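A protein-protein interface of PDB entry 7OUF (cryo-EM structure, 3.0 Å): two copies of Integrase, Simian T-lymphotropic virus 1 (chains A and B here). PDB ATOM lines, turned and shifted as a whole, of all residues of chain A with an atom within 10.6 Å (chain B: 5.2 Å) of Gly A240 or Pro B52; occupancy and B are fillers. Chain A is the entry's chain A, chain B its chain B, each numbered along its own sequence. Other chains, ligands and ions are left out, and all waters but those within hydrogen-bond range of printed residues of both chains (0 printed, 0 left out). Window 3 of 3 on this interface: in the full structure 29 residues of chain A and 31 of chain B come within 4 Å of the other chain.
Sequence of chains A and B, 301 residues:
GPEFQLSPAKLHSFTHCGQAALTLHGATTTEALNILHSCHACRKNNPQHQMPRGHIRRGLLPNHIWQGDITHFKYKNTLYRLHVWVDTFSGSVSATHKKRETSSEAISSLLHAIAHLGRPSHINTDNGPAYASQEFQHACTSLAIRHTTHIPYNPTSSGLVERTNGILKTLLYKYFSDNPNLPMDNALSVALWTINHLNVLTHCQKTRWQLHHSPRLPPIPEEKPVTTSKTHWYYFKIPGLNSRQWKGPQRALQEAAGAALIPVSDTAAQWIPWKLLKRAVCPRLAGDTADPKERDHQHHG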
ATOM      1  N   PHE A 236     -20.449   5.361 -24.991  1.00  0.00           N
ATOM      2  CA  PHE A 236     -19.632   6.266 -25.781  1.00  0.00           C
ATOM      3  C   PHE A 236     -20.507   7.206 -26.596  1.00  0.00           C
ATOM      4  O   PHE A 236     -21.690   6.949 -26.830  1.00  0.00           O
ATOM      5  CB  PHE A 236     -18.682   5.496 -26.709  1.00  0.00           C
ATOM      6  CG  PHE A 236     -19.381   4.725 -27.788  1.00  0.00           C
ATOM      7  CD1 PHE A 236     -19.924   3.481 -27.527  1.00  0.00           C
ATOM      8  CD2 PHE A 236     -19.489   5.242 -29.066  1.00  0.00           C
ATOM      9  CE1 PHE A 236     -20.562   2.770 -28.517  1.00  0.00           C
ATOM     10  CE2 PHE A 236     -20.130   4.536 -30.059  1.00  0.00           C
ATOM     11  CZ  PHE A 236     -20.666   3.298 -29.784  1.00  0.00           C
ATOM     12  N   LYS A 237     -19.897   8.312 -27.017  1.00  0.00           N
ATOM     13  CA  LYS A 237     -20.497   9.259 -27.942  1.00  0.00           C
ATOM     14  C   LYS A 237     -19.504   9.551 -29.055  1.00  0.00           C
ATOM     15  O   LYS A 237     -18.304   9.691 -28.814  1.00  0.00           O
ATOM     16  CB  LYS A 237     -20.897  10.562 -27.238  1.00  0.00           C
ATOM     17  CG  LYS A 237     -21.941  10.378 -26.153  1.00  0.00           C
ATOM     18  CD  LYS A 237     -22.599  11.691 -25.778  1.00  0.00           C
ATOM     19  CE  LYS A 237     -21.666  12.561 -24.961  1.00  0.00           C
ATOM     20  NZ  LYS A 237     -22.376  13.737 -24.392  1.00  0.00           N
ATOM     21  N   ILE A 238     -20.011   9.639 -30.276  1.00  0.00           N
ATOM     22  CA  ILE A 238     -19.145   9.849 -31.438  1.00  0.00           C
ATOM     23  C   ILE A 238     -18.711  11.311 -31.472  1.00  0.00           C
ATOM     24  O   ILE A 238     -19.568  12.205 -31.392  1.00  0.00           O
ATOM     25  CB  ILE A 238     -19.858   9.453 -32.728  1.00  0.00           C
ATOM     26  CG1 ILE A 238     -20.200   7.961 -32.731  1.00  0.00           C
ATOM     27  CG2 ILE A 238     -18.994   9.781 -33.931  1.00  0.00           C
ATOM     28  CD1 ILE A 238     -21.543   7.620 -32.122  1.00  0.00           C
ATOM     29  N   PRO A 239     -17.413  11.592 -31.572  1.00  0.00           N
ATOM     30  CA  PRO A 239     -16.959  12.986 -31.605  1.00  0.00           C
ATOM     31  C   PRO A 239     -17.486  13.725 -32.825  1.00  0.00           C
ATOM     32  O   PRO A 239     -17.644  13.151 -33.904  1.00  0.00           O
ATOM     33  CB  PRO A 239     -15.432  12.860 -31.644  1.00  0.00           C
ATOM     34  CG  PRO A 239     -15.141  11.484 -31.155  1.00  0.00           C
ATOM     35  CD  PRO A 239     -16.291  10.643 -31.590  1.00  0.00           C
ATOM     36  N   GLY A 240     -17.749  15.018 -32.645  1.00  0.00           N
ATOM     37  CA  GLY A 240     -18.180  15.862 -33.740  1.00  0.00           C
ATOM     38  C   GLY A 240     -19.643  15.774 -34.102  1.00  0.00           C
ATOM     39  O   GLY A 240     -20.008  16.121 -35.229  1.00  0.00           O
ATOM     40  N   LEU A 241     -20.499  15.311 -33.190  1.00  0.00           N
ATOM     41  CA  LEU A 241     -21.926  15.213 -33.454  1.00  0.00           C
ATOM     42  C   LEU A 241     -22.801  16.021 -32.508  1.00  0.00           C
ATOM     43  O   LEU A 241     -23.978  16.226 -32.821  1.00  0.00           O
ATOM     44  CB  LEU A 241     -22.392  13.748 -33.406  1.00  0.00           C
ATOM     45  CG  LEU A 241     -22.227  12.854 -34.640  1.00  0.00           C
ATOM     46  CD1 LEU A 241     -23.074  13.389 -35.784  1.00  0.00           C
ATOM     47  CD2 LEU A 241     -20.780  12.701 -35.069  1.00  0.00           C
ATOM     48  N   ASN A 242     -22.267  16.486 -31.377  1.00  0.00           N
ATOM     49  CA  ASN A 242     -23.052  17.188 -30.360  1.00  0.00           C
ATOM     50  C   ASN A 242     -24.255  16.354 -29.926  1.00  0.00           C
ATOM     51  O   ASN A 242     -25.378  16.850 -29.827  1.00  0.00           O
ATOM     52  CB  ASN A 242     -23.499  18.570 -30.841  1.00  0.00           C
ATOM     53  CG  ASN A 242     -23.806  19.517 -29.694  1.00  0.00           C
ATOM     54  OD1 ASN A 242     -23.428  20.686 -29.715  1.00  0.00           O
ATOM     55  ND2 ASN A 242     -24.481  19.008 -28.677  1.00  0.00           N
ATOM     56  N   SER A 243     -24.025  15.069 -29.694  1.00  0.00           N
ATOM     57  CA  SER A 243     -25.085  14.208 -29.204  1.00  0.00           C
ATOM     58  C   SER A 243     -25.173  14.297 -27.684  1.00  0.00           C
ATOM     59  O   SER A 243     -24.274  14.803 -27.007  1.00  0.00           O
ATOM     60  CB  SER A 243     -24.852  12.768 -29.652  1.00  0.00           C
ATOM     61  OG  SER A 243     -24.917  12.664 -31.064  1.00  0.00           O
ATOM     62  N   ARG A 244     -26.286  13.800 -27.143  1.00  0.00           N
ATOM     63  CA  ARG A 244     -26.529  13.835 -25.706  1.00  0.00           C
ATOM     64  C   ARG A 244     -27.041  12.500 -25.180  1.00  0.00           C
ATOM     65  O   ARG A 244     -27.512  12.430 -24.042  1.00  0.00           O
ATOM     66  CB  ARG A 244     -27.514  14.952 -25.358  1.00  0.00           C
ATOM     67  CG  ARG A 244     -26.980  16.352 -25.603  1.00  0.00           C
ATOM     68  CD  ARG A 244     -28.024  17.396 -25.264  1.00  0.00           C
ATOM     69  NE  ARG A 244     -28.339  17.434 -23.841  1.00  0.00           N
ATOM     70  CZ  ARG A 244     -29.330  18.142 -23.318  1.00  0.00           C
ATOM     71  NH1 ARG A 244     -30.111  18.897 -24.071  1.00  0.00           N
ATOM     72  NH2 ARG A 244     -29.547  18.086 -22.009  1.00  0.00           N
ATOM     73  N   GLN A 270     -12.670   3.141 -33.620  1.00  0.00           N
ATOM     74  CA  GLN A 270     -12.276   4.534 -33.485  1.00  0.00           C
ATOM     75  C   GLN A 270     -11.736   4.790 -32.086  1.00  0.00           C
ATOM     76  O   GLN A 270     -12.121   4.127 -31.119  1.00  0.00           O
ATOM     77  CB  GLN A 270     -13.454   5.471 -33.778  1.00  0.00           C
ATOM     78  CG  GLN A 270     -13.053   6.897 -34.089  1.00  0.00           C
ATOM     79  CD  GLN A 270     -14.245   7.808 -34.253  1.00  0.00           C
ATOM     80  OE1 GLN A 270     -15.302   7.386 -34.720  1.00  0.00           O
ATOM     81  NE2 GLN A 270     -14.083   9.070 -33.875  1.00  0.00           N
ATOM     82  N   TRP A 271     -10.837   5.767 -31.991  1.00  0.00           N
ATOM     83  CA  TRP A 271     -10.281   6.197 -30.713  1.00  0.00           C
ATOM     84  C   TRP A 271     -11.168   7.303 -30.150  1.00  0.00           C
ATOM     85  O   TRP A 271     -11.155   8.432 -30.646  1.00  0.00           O
ATOM     86  CB  TRP A 271      -8.842   6.674 -30.884  1.00  0.00           C
ATOM     87  CG  TRP A 271      -7.852   5.562 -31.042  1.00  0.00           C
ATOM     88  CD1 TRP A 271      -7.322   5.099 -32.206  1.00  0.00           C
ATOM     89  CD2 TRP A 271      -7.271   4.776 -29.997  1.00  0.00           C
ATOM     90  NE1 TRP A 271      -6.448   4.072 -31.955  1.00  0.00           N
ATOM     91  CE2 TRP A 271      -6.400   3.854 -30.604  1.00  0.00           C
ATOM     92  CE3 TRP A 271      -7.404   4.761 -28.606  1.00  0.00           C
ATOM     93  CZ2 TRP A 271      -5.664   2.929 -29.871  1.00  0.00           C
ATOM     94  CZ3 TRP A 271      -6.673   3.841 -27.882  1.00  0.00           C
ATOM     95  CH2 TRP A 271      -5.815   2.939 -28.515  1.00  0.00           C
ATOM     96  N   ILE A 272     -11.936   6.975 -29.122  1.00  0.00           N
ATOM     97  CA  ILE A 272     -12.870   7.905 -28.495  1.00  0.00           C
ATOM     98  C   ILE A 272     -12.192   8.510 -27.272  1.00  0.00           C
ATOM     99  O   ILE A 272     -11.604   7.764 -26.477  1.00  0.00           O
ATOM    100  CB  ILE A 272     -14.183   7.207 -28.098  1.00  0.00           C
ATOM    101  CG1 ILE A 272     -14.726   6.381 -29.266  1.00  0.00           C
ATOM    102  CG2 ILE A 272     -15.212   8.224 -27.638  1.00  0.00           C
ATOM    103  CD1 ILE A 272     -15.118   7.203 -30.469  1.00  0.00           C
ATOM    104  N   PRO A 273     -12.241   9.827 -27.088  1.00  0.00           N
ATOM    105  CA  PRO A 273     -11.617  10.436 -25.910  1.00  0.00           C
ATOM    106  C   PRO A 273     -12.333  10.049 -24.624  1.00  0.00           C
ATOM    107  O   PRO A 273     -13.467   9.571 -24.625  1.00  0.00           O
ATOM    108  CB  PRO A 273     -11.738  11.939 -26.180  1.00  0.00           C
ATOM    109  CG  PRO A 273     -11.941  12.047 -27.655  1.00  0.00           C
ATOM    110  CD  PRO A 273     -12.721  10.839 -28.041  1.00  0.00           C
ATOM    111  N   LEU A 276     -15.794  11.579 -23.622  1.00  0.00           N
ATOM    112  CA  LEU A 276     -16.958  11.016 -24.290  1.00  0.00           C
ATOM    113  C   LEU A 276     -17.197   9.562 -23.905  1.00  0.00           C
ATOM    114  O   LEU A 276     -17.962   8.866 -24.579  1.00  0.00           O
ATOM    115  CB  LEU A 276     -16.818  11.147 -25.806  1.00  0.00           C
ATOM    116  CG  LEU A 276     -16.814  12.565 -26.378  1.00  0.00           C
ATOM    117  CD1 LEU A 276     -16.698  12.527 -27.887  1.00  0.00           C
ATOM    118  CD2 LEU A 276     -18.065  13.312 -25.962  1.00  0.00           C
ATOM    119  N   GLN B  50     -24.592  26.740 -29.943  1.00  0.00           N
ATOM    120  CA  GLN B  50     -24.674  25.305 -29.681  1.00  0.00           C
ATOM    121  C   GLN B  50     -24.047  24.565 -30.862  1.00  0.00           C
ATOM    122  O   GLN B  50     -24.719  24.345 -31.876  1.00  0.00           O
ATOM    123  CB  GLN B  50     -26.126  24.901 -29.468  1.00  0.00           C
ATOM    124  CG  GLN B  50     -26.365  23.449 -29.106  1.00  0.00           C
ATOM    125  CD  GLN B  50     -25.730  23.055 -27.789  1.00  0.00           C
ATOM    126  OE1 GLN B  50     -26.213  23.400 -26.711  1.00  0.00           O
ATOM    127  NE2 GLN B  50     -24.637  22.306 -27.874  1.00  0.00           N
ATOM    128  N   MET B  51     -22.779  24.185 -30.724  1.00  0.00           N
ATOM    129  CA  MET B  51     -22.037  23.425 -31.719  1.00  0.00           C
ATOM    130  C   MET B  51     -21.152  22.372 -31.071  1.00  0.00           C
ATOM    131  O   MET B  51     -20.858  22.454 -29.875  1.00  0.00           O
ATOM    132  CB  MET B  51     -21.191  24.339 -32.619  1.00  0.00           C
ATOM    133  CG  MET B  51     -22.007  25.253 -33.536  1.00  0.00           C
ATOM    134  SD  MET B  51     -21.002  26.356 -34.538  1.00  0.00           S
ATOM    135  CE  MET B  51     -20.283  25.165 -35.658  1.00  0.00           C
ATOM    136  N   PRO B  52     -20.729  21.355 -31.828  1.00  0.00           N
ATOM    137  CA  PRO B  52     -19.937  20.273 -31.236  1.00  0.00           C
ATOM    138  C   PRO B  52     -18.555  20.737 -30.809  1.00  0.00           C
ATOM    139  O   PRO B  52     -18.046  21.773 -31.240  1.00  0.00           O
ATOM    140  CB  PRO B  52     -19.849  19.237 -32.360  1.00  0.00           C
ATOM    141  CG  PRO B  52     -20.895  19.603 -33.320  1.00  0.00           C
ATOM    142  CD  PRO B  52     -21.052  21.075 -33.239  1.00  0.00           C
ATOM    143  N   ARG B  53     -17.961  19.942 -29.928  1.00  0.00           N
ATOM    144  CA  ARG B  53     -16.633  20.192 -29.394  1.00  0.00           C
ATOM    145  C   ARG B  53     -15.565  19.573 -30.288  1.00  0.00           C
ATOM    146  O   ARG B  53     -15.821  18.630 -31.040  1.00  0.00           O
ATOM    147  CB  ARG B  53     -16.502  19.622 -27.981  1.00  0.00           C
ATOM    148  CG  ARG B  53     -17.639  19.983 -27.052  1.00  0.00           C
ATOM    149  CD  ARG B  53     -17.371  19.474 -25.645  1.00  0.00           C
ATOM    150  NE  ARG B  53     -16.351  20.250 -24.951  1.00  0.00           N
ATOM    151  CZ  ARG B  53     -16.403  20.578 -23.666  1.00  0.00           C
ATOM    152  NH1 ARG B  53     -17.417  20.211 -22.900  1.00  0.00           N
ATOM    153  NH2 ARG B  53     -15.419  21.300 -23.140  1.00  0.00           N
ATOM    154  N   GLY B  54     -14.356  20.123 -30.195  1.00  0.00           N
ATOM    155  CA  GLY B  54     -13.211  19.599 -30.914  1.00  0.00           C
ATOM    156  C   GLY B  54     -12.225  18.894 -30.004  1.00  0.00           C
ATOM    157  O   GLY B  54     -12.199  19.143 -28.796  1.00  0.00           O
ATOM    158  N   HIS B  55     -11.415  18.005 -30.572  1.00  0.00           N
ATOM    159  CA  HIS B  55     -10.414  17.263 -29.818  1.00  0.00           C
ATOM    160  C   HIS B  55      -9.114  17.226 -30.604  1.00  0.00           C
ATOM    161  O   HIS B  55      -9.127  17.023 -31.818  1.00  0.00           O
ATOM    162  CB  HIS B  55     -10.884  15.837 -29.529  1.00  0.00           C
ATOM    163  CG  HIS B  55     -12.270  15.761 -28.972  1.00  0.00           C
ATOM    164  ND1 HIS B  55     -13.338  15.291 -29.702  1.00  0.00           N
ATOM    165  CD2 HIS B  55     -12.761  16.085 -27.754  1.00  0.00           C
ATOM    166  CE1 HIS B  55     -14.430  15.335 -28.961  1.00  0.00           C
ATOM    167  NE2 HIS B  55     -14.106  15.812 -27.773  1.00  0.00           N
ATOM    168  N   TRP B 274     -14.598  25.438 -34.292  1.00  0.00           N
ATOM    169  CA  TRP B 274     -16.034  25.289 -34.104  1.00  0.00           C
ATOM    170  C   TRP B 274     -16.561  26.119 -32.943  1.00  0.00           C
ATOM    171  O   TRP B 274     -17.739  26.485 -32.944  1.00  0.00           O
ATOM    172  CB  TRP B 274     -16.385  23.818 -33.876  1.00  0.00           C
ATOM    173  CG  TRP B 274     -16.588  23.030 -35.134  1.00  0.00           C
ATOM    174  CD1 TRP B 274     -16.778  23.524 -36.390  1.00  0.00           C
ATOM    175  CD2 TRP B 274     -16.629  21.605 -35.254  1.00  0.00           C
ATOM    176  NE1 TRP B 274     -16.930  22.495 -37.285  1.00  0.00           N
ATOM    177  CE2 TRP B 274     -16.843  21.306 -36.612  1.00  0.00           C
ATOM    178  CE3 TRP B 274     -16.503  20.551 -34.344  1.00  0.00           C
ATOM    179  CZ2 TRP B 274     -16.934  20.000 -37.082  1.00  0.00           C
ATOM    180  CZ3 TRP B 274     -16.592  19.256 -34.812  1.00  0.00           C
ATOM    181  CH2 TRP B 274     -16.807  18.990 -36.167  1.00  0.00           C
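The side-chain amide nitrogen (NE2) of Gln B50 sits at hydrogen-bond distance from the side-chain amide oxygen (OD1) of Asn A242.
The backbone carbonyl oxygen (O) of Met B51 sits close to the side-chain amide oxygen (OD1) of Asn A242, at 3.1 Å.
N of Pro B52 lies close to OD1 of Asn A242 (3.5 Å).
Pro A239 touches His B55.
Pro B52 touches Gly A240 (CB to C, 3.9 Å).
Trp B274 touches Gly A240 (CZ3 to CA, 3.9 Å).
Pro A273 touches His B55.
Leu A276 touches His B55 (CD1 to CE1, 3.8 Å).
N of Lys A237 is in hydrogen-bond range of O of Leu A276, at 3.2 Å.
No position is printed for both chains.
Of the 8 pairs that touch across the chains among the printed residues, none has its exchanged pair printed and touching as well.
Gly A240 touches two residues of chain B.
Of chain A, only Gly A240 and Asn A242 come within 4 Å of Pro B52.
Of chain A, only Asn A242 comes within 4 Å of Met B51.
Trp B274 touches one residue of chain A.
Of the printed residues of chain B, Pro A239 touches His B55.
Printed residues of chain A within 4 Å of His B55: Pro A239 (3.8 Å), Pro A273 (3.95 Å) and Leu A276 (3.8 Å).
Of the printed residues of chain B, Leu A276 touches His B55.
Of the printed residues of chain B, Asn A242 touches Gln B50 (2.7 Å), Met B51 (3.1 Å) and Pro B52 (3.5 Å).
Of the printed residues of chain A, Gln B50 touches Asn A242.
Arg B53 touches none of the printed residues of chain A.
Gly B54 touches none of the printed residues of chain A.
The nearest residue of chain B that does not touch Gly A240 is Arg B53 (4.4 Å).
The nearest residue of chain A that does not touch Pro B52 is Leu A241 (4.1 Å).
Of the 14 printed residues of chain A, 5 touch a printed residue of chain B.
Printed residues of chain A that touch a printed residue of chain B: Pro A239, Gly A240, Asn A242, Pro A273 and Leu A276.
Hydrophobic or aromatic side chains of chain A within 4 Å of the printed part of chain B: Pro A239, Pro A273 and Leu A276.
Of the 7 printed residues of chain B, 5 touch a printed residue of chain A.
Among the printed residues, no Asp or Glu carboxylate lies within 4 Å of a Lys or Arg side-chain nitrogen of the other chain.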
